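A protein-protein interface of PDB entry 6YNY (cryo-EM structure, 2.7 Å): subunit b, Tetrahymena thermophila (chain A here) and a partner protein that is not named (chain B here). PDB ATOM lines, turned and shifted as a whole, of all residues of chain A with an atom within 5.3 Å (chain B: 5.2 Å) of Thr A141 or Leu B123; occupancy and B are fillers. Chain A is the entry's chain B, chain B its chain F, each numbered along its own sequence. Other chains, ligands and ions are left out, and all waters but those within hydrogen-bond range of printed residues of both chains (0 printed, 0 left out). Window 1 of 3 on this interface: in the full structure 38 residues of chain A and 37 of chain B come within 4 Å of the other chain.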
ATOM      1  N   TRP A 136      15.457  34.211   1.098  1.00  0.00           N
ATOM      2  CA  TRP A 136      15.295  32.982   0.336  1.00  0.00           C
ATOM      3  C   TRP A 136      15.856  31.783   1.086  1.00  0.00           C
ATOM      4  O   TRP A 136      15.365  30.661   0.913  1.00  0.00           O
ATOM      5  CB  TRP A 136      15.974  33.140  -1.019  1.00  0.00           C
ATOM      6  CG  TRP A 136      15.949  31.933  -1.880  1.00  0.00           C
ATOM      7  CD1 TRP A 136      14.939  31.527  -2.692  1.00  0.00           C
ATOM      8  CD2 TRP A 136      16.996  30.975  -2.033  1.00  0.00           C
ATOM      9  NE1 TRP A 136      15.286  30.372  -3.337  1.00  0.00           N
ATOM     10  CE2 TRP A 136      16.547  30.012  -2.950  1.00  0.00           C
ATOM     11  CE3 TRP A 136      18.268  30.838  -1.481  1.00  0.00           C
ATOM     12  CZ2 TRP A 136      17.325  28.927  -3.322  1.00  0.00           C
ATOM     13  CZ3 TRP A 136      19.034  29.763  -1.853  1.00  0.00           C
ATOM     14  CH2 TRP A 136      18.563  28.821  -2.765  1.00  0.00           C
ATOM     15  N   ILE A 137      16.869  31.997   1.922  1.00  0.00           N
ATOM     16  CA  ILE A 137      17.430  30.910   2.713  1.00  0.00           C
ATOM     17  C   ILE A 137      16.527  30.575   3.891  1.00  0.00           C
ATOM     18  O   ILE A 137      16.323  29.402   4.215  1.00  0.00           O
ATOM     19  CB  ILE A 137      18.850  31.283   3.170  1.00  0.00           C
ATOM     20  CG1 ILE A 137      19.783  31.327   1.963  1.00  0.00           C
ATOM     21  CG2 ILE A 137      19.358  30.305   4.206  1.00  0.00           C
ATOM     22  CD1 ILE A 137      21.160  31.806   2.268  1.00  0.00           C
ATOM     23  N   MET A 138      15.980  31.592   4.557  1.00  0.00           N
ATOM     24  CA  MET A 138      15.086  31.344   5.681  1.00  0.00           C
ATOM     25  C   MET A 138      13.833  30.603   5.231  1.00  0.00           C
ATOM     26  O   MET A 138      13.400  29.642   5.874  1.00  0.00           O
ATOM     27  CB  MET A 138      14.716  32.663   6.355  1.00  0.00           C
ATOM     28  CG  MET A 138      15.865  33.387   7.018  1.00  0.00           C
ATOM     29  SD  MET A 138      16.442  32.599   8.525  1.00  0.00           S
ATOM     30  CE  MET A 138      17.379  33.944   9.235  1.00  0.00           C
ATOM     31  N   LYS A 139      13.233  31.045   4.126  1.00  0.00           N
ATOM     32  CA  LYS A 139      12.052  30.369   3.603  1.00  0.00           C
ATOM     33  C   LYS A 139      12.383  28.966   3.115  1.00  0.00           C
ATOM     34  O   LYS A 139      11.582  28.042   3.282  1.00  0.00           O
ATOM     35  CB  LYS A 139      11.436  31.198   2.479  1.00  0.00           C
ATOM     36  CG  LYS A 139      10.730  32.442   2.951  1.00  0.00           C
ATOM     37  CD  LYS A 139      10.281  33.311   1.804  1.00  0.00           C
ATOM     38  CE  LYS A 139       9.413  34.443   2.299  1.00  0.00           C
ATOM     39  NZ  LYS A 139       8.941  35.312   1.207  1.00  0.00           N
ATOM     40  N   SER A 140      13.558  28.786   2.515  1.00  0.00           N
ATOM     41  CA  SER A 140      13.955  27.469   2.041  1.00  0.00           C
ATOM     42  C   SER A 140      14.248  26.504   3.180  1.00  0.00           C
ATOM     43  O   SER A 140      14.285  25.292   2.954  1.00  0.00           O
ATOM     44  CB  SER A 140      15.181  27.593   1.141  1.00  0.00           C
ATOM     45  OG  SER A 140      14.975  28.555   0.130  1.00  0.00           O
ATOM     46  N   THR A 141      14.455  27.013   4.394  1.00  0.00           N
ATOM     47  CA  THR A 141      14.773  26.191   5.550  1.00  0.00           C
ATOM     48  C   THR A 141      13.554  25.856   6.400  1.00  0.00           C
ATOM     49  O   THR A 141      13.663  25.033   7.313  1.00  0.00           O
ATOM     50  CB  THR A 141      15.820  26.903   6.418  1.00  0.00           C
ATOM     51  OG1 THR A 141      16.957  27.241   5.618  1.00  0.00           O
ATOM     52  CG2 THR A 141      16.268  26.033   7.567  1.00  0.00           C
ATOM     53  N   TYR A 142      12.398  26.450   6.111  1.00  0.00           N
ATOM     54  CA  TYR A 142      11.226  26.244   6.953  1.00  0.00           C
ATOM     55  C   TYR A 142      10.753  24.797   6.912  1.00  0.00           C
ATOM     56  O   TYR A 142      10.554  24.171   7.957  1.00  0.00           O
ATOM     57  CB  TYR A 142      10.106  27.189   6.525  1.00  0.00           C
ATOM     58  CG  TYR A 142       8.819  26.996   7.279  1.00  0.00           C
ATOM     59  CD1 TYR A 142       8.655  27.514   8.551  1.00  0.00           C
ATOM     60  CD2 TYR A 142       7.765  26.299   6.717  1.00  0.00           C
ATOM     61  CE1 TYR A 142       7.486  27.339   9.239  1.00  0.00           C
ATOM     62  CE2 TYR A 142       6.593  26.118   7.398  1.00  0.00           C
ATOM     63  CZ  TYR A 142       6.455  26.640   8.660  1.00  0.00           C
ATOM     64  OH  TYR A 142       5.280  26.462   9.345  1.00  0.00           O
ATOM     65  N   ILE A 143      10.564  24.249   5.712  1.00  0.00           N
ATOM     66  CA  ILE A 143      10.039  22.889   5.596  1.00  0.00           C
ATOM     67  C   ILE A 143      10.904  21.880   6.339  1.00  0.00           C
ATOM     68  O   ILE A 143      10.369  21.142   7.181  1.00  0.00           O
ATOM     69  CB  ILE A 143       9.843  22.523   4.114  1.00  0.00           C
ATOM     70  CG1 ILE A 143       8.671  23.313   3.529  1.00  0.00           C
ATOM     71  CG2 ILE A 143       9.611  21.038   3.967  1.00  0.00           C
ATOM     72  CD1 ILE A 143       8.487  23.150   2.046  1.00  0.00           C
ATOM     73  N   PRO A 144      12.211  21.781   6.089  1.00  0.00           N
ATOM     74  CA  PRO A 144      13.009  20.783   6.817  1.00  0.00           C
ATOM     75  C   PRO A 144      13.074  21.029   8.311  1.00  0.00           C
ATOM     76  O   PRO A 144      13.226  20.072   9.079  1.00  0.00           O
ATOM     77  CB  PRO A 144      14.390  20.891   6.159  1.00  0.00           C
ATOM     78  CG  PRO A 144      14.409  22.200   5.495  1.00  0.00           C
ATOM     79  CD  PRO A 144      13.011  22.495   5.085  1.00  0.00           C
ATOM     80  N   TRP A 145      12.971  22.281   8.750  1.00  0.00           N
ATOM     81  CA  TRP A 145      12.965  22.562  10.181  1.00  0.00           C
ATOM     82  C   TRP A 145      11.734  21.965  10.849  1.00  0.00           C
ATOM     83  O   TRP A 145      11.822  21.420  11.954  1.00  0.00           O
ATOM     84  CB  TRP A 145      13.031  24.068  10.413  1.00  0.00           C
ATOM     85  CG  TRP A 145      13.209  24.449  11.836  1.00  0.00           C
ATOM     86  CD1 TRP A 145      12.235  24.788  12.717  1.00  0.00           C
ATOM     87  CD2 TRP A 145      14.443  24.528  12.551  1.00  0.00           C
ATOM     88  NE1 TRP A 145      12.780  25.074  13.937  1.00  0.00           N
ATOM     89  CE2 TRP A 145      14.136  24.923  13.862  1.00  0.00           C
ATOM     90  CE3 TRP A 145      15.776  24.305  12.210  1.00  0.00           C
ATOM     91  CZ2 TRP A 145      15.112  25.095  14.831  1.00  0.00           C
ATOM     92  CZ3 TRP A 145      16.741  24.479  13.172  1.00  0.00           C
ATOM     93  CH2 TRP A 145      16.405  24.870  14.466  1.00  0.00           C
ATOM     94  N   ILE A 146      10.580  22.054  10.192  1.00  0.00           N
ATOM     95  CA  ILE A 146       9.363  21.484  10.757  1.00  0.00           C
ATOM     96  C   ILE A 146       9.391  19.965  10.659  1.00  0.00           C
ATOM     97  O   ILE A 146       8.993  19.262  11.593  1.00  0.00           O
ATOM     98  CB  ILE A 146       8.124  22.064  10.053  1.00  0.00           C
ATOM     99  CG1 ILE A 146       8.090  23.590  10.161  1.00  0.00           C
ATOM    100  CG2 ILE A 146       6.871  21.465  10.624  1.00  0.00           C
ATOM    101  CD1 ILE A 146       8.059  24.121  11.555  1.00  0.00           C
ATOM    102  N   PHE B 116      21.594  20.297   9.113  1.00  0.00           N
ATOM    103  CA  PHE B 116      21.136  21.676   8.994  1.00  0.00           C
ATOM    104  C   PHE B 116      22.293  22.626   8.726  1.00  0.00           C
ATOM    105  O   PHE B 116      22.142  23.601   7.982  1.00  0.00           O
ATOM    106  CB  PHE B 116      20.386  22.089  10.259  1.00  0.00           C
ATOM    107  CG  PHE B 116      18.977  21.603  10.305  1.00  0.00           C
ATOM    108  CD1 PHE B 116      17.959  22.355   9.760  1.00  0.00           C
ATOM    109  CD2 PHE B 116      18.666  20.395  10.889  1.00  0.00           C
ATOM    110  CE1 PHE B 116      16.667  21.913   9.798  1.00  0.00           C
ATOM    111  CE2 PHE B 116      17.372  19.950  10.928  1.00  0.00           C
ATOM    112  CZ  PHE B 116      16.372  20.710  10.382  1.00  0.00           C
ATOM    113  N   LEU B 118      25.197  21.898   7.130  1.00  0.00           N
ATOM    114  CA  LEU B 118      25.618  21.729   5.745  1.00  0.00           C
ATOM    115  C   LEU B 118      24.536  22.184   4.777  1.00  0.00           C
ATOM    116  O   LEU B 118      24.835  22.797   3.746  1.00  0.00           O
ATOM    117  CB  LEU B 118      25.983  20.274   5.483  1.00  0.00           C
ATOM    118  CG  LEU B 118      27.171  19.721   6.262  1.00  0.00           C
ATOM    119  CD1 LEU B 118      27.412  18.293   5.879  1.00  0.00           C
ATOM    120  CD2 LEU B 118      28.406  20.553   6.024  1.00  0.00           C
ATOM    121  N   GLY B 119      23.276  21.886   5.084  1.00  0.00           N
ATOM    122  CA  GLY B 119      22.194  22.352   4.239  1.00  0.00           C
ATOM    123  C   GLY B 119      22.130  23.860   4.151  1.00  0.00           C
ATOM    124  O   GLY B 119      21.757  24.412   3.114  1.00  0.00           O
ATOM    125  N   PHE B 120      22.494  24.546   5.232  1.00  0.00           N
ATOM    126  CA  PHE B 120      22.545  26.000   5.206  1.00  0.00           C
ATOM    127  C   PHE B 120      23.687  26.485   4.326  1.00  0.00           C
ATOM    128  O   PHE B 120      23.542  27.467   3.590  1.00  0.00           O
ATOM    129  CB  PHE B 120      22.685  26.524   6.631  1.00  0.00           C
ATOM    130  CG  PHE B 120      22.538  28.003   6.751  1.00  0.00           C
ATOM    131  CD1 PHE B 120      21.289  28.573   6.893  1.00  0.00           C
ATOM    132  CD2 PHE B 120      23.643  28.824   6.733  1.00  0.00           C
ATOM    133  CE1 PHE B 120      21.148  29.932   7.009  1.00  0.00           C
ATOM    134  CE2 PHE B 120      23.507  30.181   6.848  1.00  0.00           C
ATOM    135  CZ  PHE B 120      22.258  30.739   6.987  1.00  0.00           C
ATOM    136  N   ILE B 121      24.829  25.802   4.385  1.00  0.00           N
ATOM    137  CA  ILE B 121      25.959  26.148   3.534  1.00  0.00           C
ATOM    138  C   ILE B 121      25.648  25.845   2.078  1.00  0.00           C
ATOM    139  O   ILE B 121      26.098  26.561   1.176  1.00  0.00           O
ATOM    140  CB  ILE B 121      27.214  25.397   4.009  1.00  0.00           C
ATOM    141  CG1 ILE B 121      27.621  25.881   5.398  1.00  0.00           C
ATOM    142  CG2 ILE B 121      28.338  25.573   3.022  1.00  0.00           C
ATOM    143  CD1 ILE B 121      28.638  25.005   6.078  1.00  0.00           C
ATOM    144  N   LYS B 122      24.883  24.786   1.822  1.00  0.00           N
ATOM    145  CA  LYS B 122      24.513  24.449   0.455  1.00  0.00           C
ATOM    146  C   LYS B 122      23.657  25.545  -0.166  1.00  0.00           C
ATOM    147  O   LYS B 122      23.867  25.928  -1.322  1.00  0.00           O
ATOM    148  CB  LYS B 122      23.777  23.114   0.444  1.00  0.00           C
ATOM    149  CG  LYS B 122      23.577  22.523  -0.929  1.00  0.00           C
ATOM    150  CD  LYS B 122      22.760  21.246  -0.879  1.00  0.00           C
ATOM    151  CE  LYS B 122      23.455  20.147  -0.098  1.00  0.00           C
ATOM    152  NZ  LYS B 122      24.798  19.863  -0.649  1.00  0.00           N
ATOM    153  N   LEU B 123      22.691  26.067   0.589  1.00  0.00           N
ATOM    154  CA  LEU B 123      21.858  27.149   0.080  1.00  0.00           C
ATOM    155  C   LEU B 123      22.659  28.429  -0.096  1.00  0.00           C
ATOM    156  O   LEU B 123      22.420  29.194  -1.036  1.00  0.00           O
ATOM    157  CB  LEU B 123      20.680  27.387   1.019  1.00  0.00           C
ATOM    158  CG  LEU B 123      19.716  26.227   1.228  1.00  0.00           C
ATOM    159  CD1 LEU B 123      18.690  26.603   2.258  1.00  0.00           C
ATOM    160  CD2 LEU B 123      19.043  25.844  -0.063  1.00  0.00           C
ATOM    161  N   LYS B 124      23.610  28.682   0.801  1.00  0.00           N
ATOM    162  CA  LYS B 124      24.471  29.848   0.653  1.00  0.00           C
ATOM    163  C   LYS B 124      25.292  29.762  -0.626  1.00  0.00           C
ATOM    164  O   LYS B 124      25.516  30.774  -1.298  1.00  0.00           O
ATOM    165  CB  LYS B 124      25.376  29.967   1.876  1.00  0.00           C
ATOM    166  CG  LYS B 124      26.437  31.028   1.801  1.00  0.00           C
ATOM    167  CD  LYS B 124      25.878  32.409   1.600  1.00  0.00           C
ATOM    168  CE  LYS B 124      26.991  33.431   1.636  1.00  0.00           C
ATOM    169  NZ  LYS B 124      26.509  34.793   1.352  1.00  0.00           N
ATOM    170  N   ALA B 125      25.738  28.560  -0.985  1.00  0.00           N
ATOM    171  CA  ALA B 125      26.471  28.392  -2.233  1.00  0.00           C
ATOM    172  C   ALA B 125      25.577  28.648  -3.438  1.00  0.00           C
ATOM    173  O   ALA B 125      26.038  29.176  -4.457  1.00  0.00           O
ATOM    174  CB  ALA B 125      27.070  26.993  -2.299  1.00  0.00           C
ATOM    175  N   GLN B 126      24.300  28.278  -3.345  1.00  0.00           N
ATOM    176  CA  GLN B 126      23.373  28.559  -4.434  1.00  0.00           C
ATOM    177  C   GLN B 126      23.043  30.043  -4.510  1.00  0.00           C
ATOM    178  O   GLN B 126      22.873  30.590  -5.604  1.00  0.00           O
ATOM    179  CB  GLN B 126      22.097  27.741  -4.258  1.00  0.00           C
ATOM    180  CG  GLN B 126      22.303  26.250  -4.336  1.00  0.00           C
ATOM    181  CD  GLN B 126      21.009  25.485  -4.250  1.00  0.00           C
ATOM    182  OE1 GLN B 126      19.944  25.999  -4.585  1.00  0.00           O
ATOM    183  NE2 GLN B 126      21.090  24.249  -3.794  1.00  0.00           N
ATOM    184  N   SER B 127      22.950  30.708  -3.359  1.00  0.00           N
ATOM    185  CA  SER B 127      22.689  32.141  -3.357  1.00  0.00           C
ATOM    186  C   SER B 127      23.837  32.911  -3.987  1.00  0.00           C
ATOM    187  O   SER B 127      23.616  33.949  -4.618  1.00  0.00           O
ATOM    188  CB  SER B 127      22.445  32.621  -1.929  1.00  0.00           C
ATOM    189  OG  SER B 127      21.979  33.953  -1.910  1.00  0.00           O
ATOM    190  N   ILE B 128      25.064  32.421  -3.822  1.00  0.00           N
ATOM    191  CA  ILE B 128      26.212  33.044  -4.466  1.00  0.00           C
ATOM    192  C   ILE B 128      26.159  32.829  -5.970  1.00  0.00           C
ATOM    193  O   ILE B 128      26.468  33.733  -6.752  1.00  0.00           O
ATOM    194  CB  ILE B 128      27.515  32.496  -3.862  1.00  0.00           C
ATOM    195  CG1 ILE B 128      27.628  32.899  -2.397  1.00  0.00           C
ATOM    196  CG2 ILE B 128      28.713  32.996  -4.633  1.00  0.00           C
ATOM    197  CD1 ILE B 128      28.725  32.198  -1.680  1.00  0.00           C
ATOM    198  N   GLY B 160      14.007  26.548  -3.381  1.00  0.00           N
ATOM    199  CA  GLY B 160      15.131  25.698  -3.033  1.00  0.00           C
ATOM    200  C   GLY B 160      14.648  24.358  -2.518  1.00  0.00           C
ATOM    201  O   GLY B 160      13.643  24.266  -1.804  1.00  0.00           O
ATOM    202  N   MET B 161      15.376  23.313  -2.870  1.00  0.00           N
ATOM    203  CA  MET B 161      14.976  21.957  -2.548  1.00  0.00           C
ATOM    204  C   MET B 161      14.815  21.803  -1.042  1.00  0.00           C
ATOM    205  O   MET B 161      15.794  21.986  -0.303  1.00  0.00           O
ATOM    206  CB  MET B 161      16.011  20.970  -3.073  1.00  0.00           C
ATOM    207  CG  MET B 161      15.585  19.512  -3.012  1.00  0.00           C
ATOM    208  SD  MET B 161      16.948  18.370  -3.279  1.00  0.00           S
ATOM    209  CE  MET B 161      17.495  18.883  -4.901  1.00  0.00           C
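Of the 11 printed residues of chain A, 6 touch a printed residue of chain B.
Hydrophobic or aromatic side chains of chain A that line the printed part of chain B: Trp A136, Ile A137 and Trp A145.
Printed residues of chain B that touch a printed residue of chain A: Phe B116, Phe B120, Leu B123, Gln B126 and Gly B160.
Hydrophobic or aromatic side chains of chain B within 4 Å of the printed part of chain A: Phe B116, Phe B120 and Leu B123.
The backbone carbonyl oxygen of Ile A137 lies within hydrogen-bond range of the side-chain hydroxyl of Thr A141, 2.7 Å away.
Among the printed residues, merely in contact across the chains: Trp A136 with Leu B123 (3.5 Å), Trp A136 with Gln B126 (3.6 Å), Trp A136 with Gly B160 (3.9 Å), Ile A137 with Phe B120 (3.3 Å), Ser A140 with Leu B123 (3.8 Å), Thr A141 with Leu B123 (3.8 Å), Pro A144 with Phe B116 (3.5 Å) and Trp A145 with Phe B116 (3.5 Å).
Thr A141 touches just one residue of chain B: Leu B123.
Of chain A, only Trp A136, Ser A140 and Thr A141 come within 4 Å of Leu B123.
Printed residues of chain A within 4 Å of Phe B116: Pro A144 and Trp A145.
Printed residues of chain A within 4 Å of Phe B120: Ile A137.
Of the printed residues of chain B, Pro A144 touches Phe B116 (3.5 Å).
Printed residues of chain A within 4 Å of Gly B160: Trp A136 (3.9 Å).
Met A138 touches none of the printed residues of chain B.
The nearest residue of chain B that does not touch Thr A141 is Phe B116 (4.6 Å).
The nearest residue of chain A that does not touch Leu B123 is Ile A137 (4.1 Å).
The nearest printed residue of chain B that does not touch Trp A145 is Phe B120 (8.8 Å).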
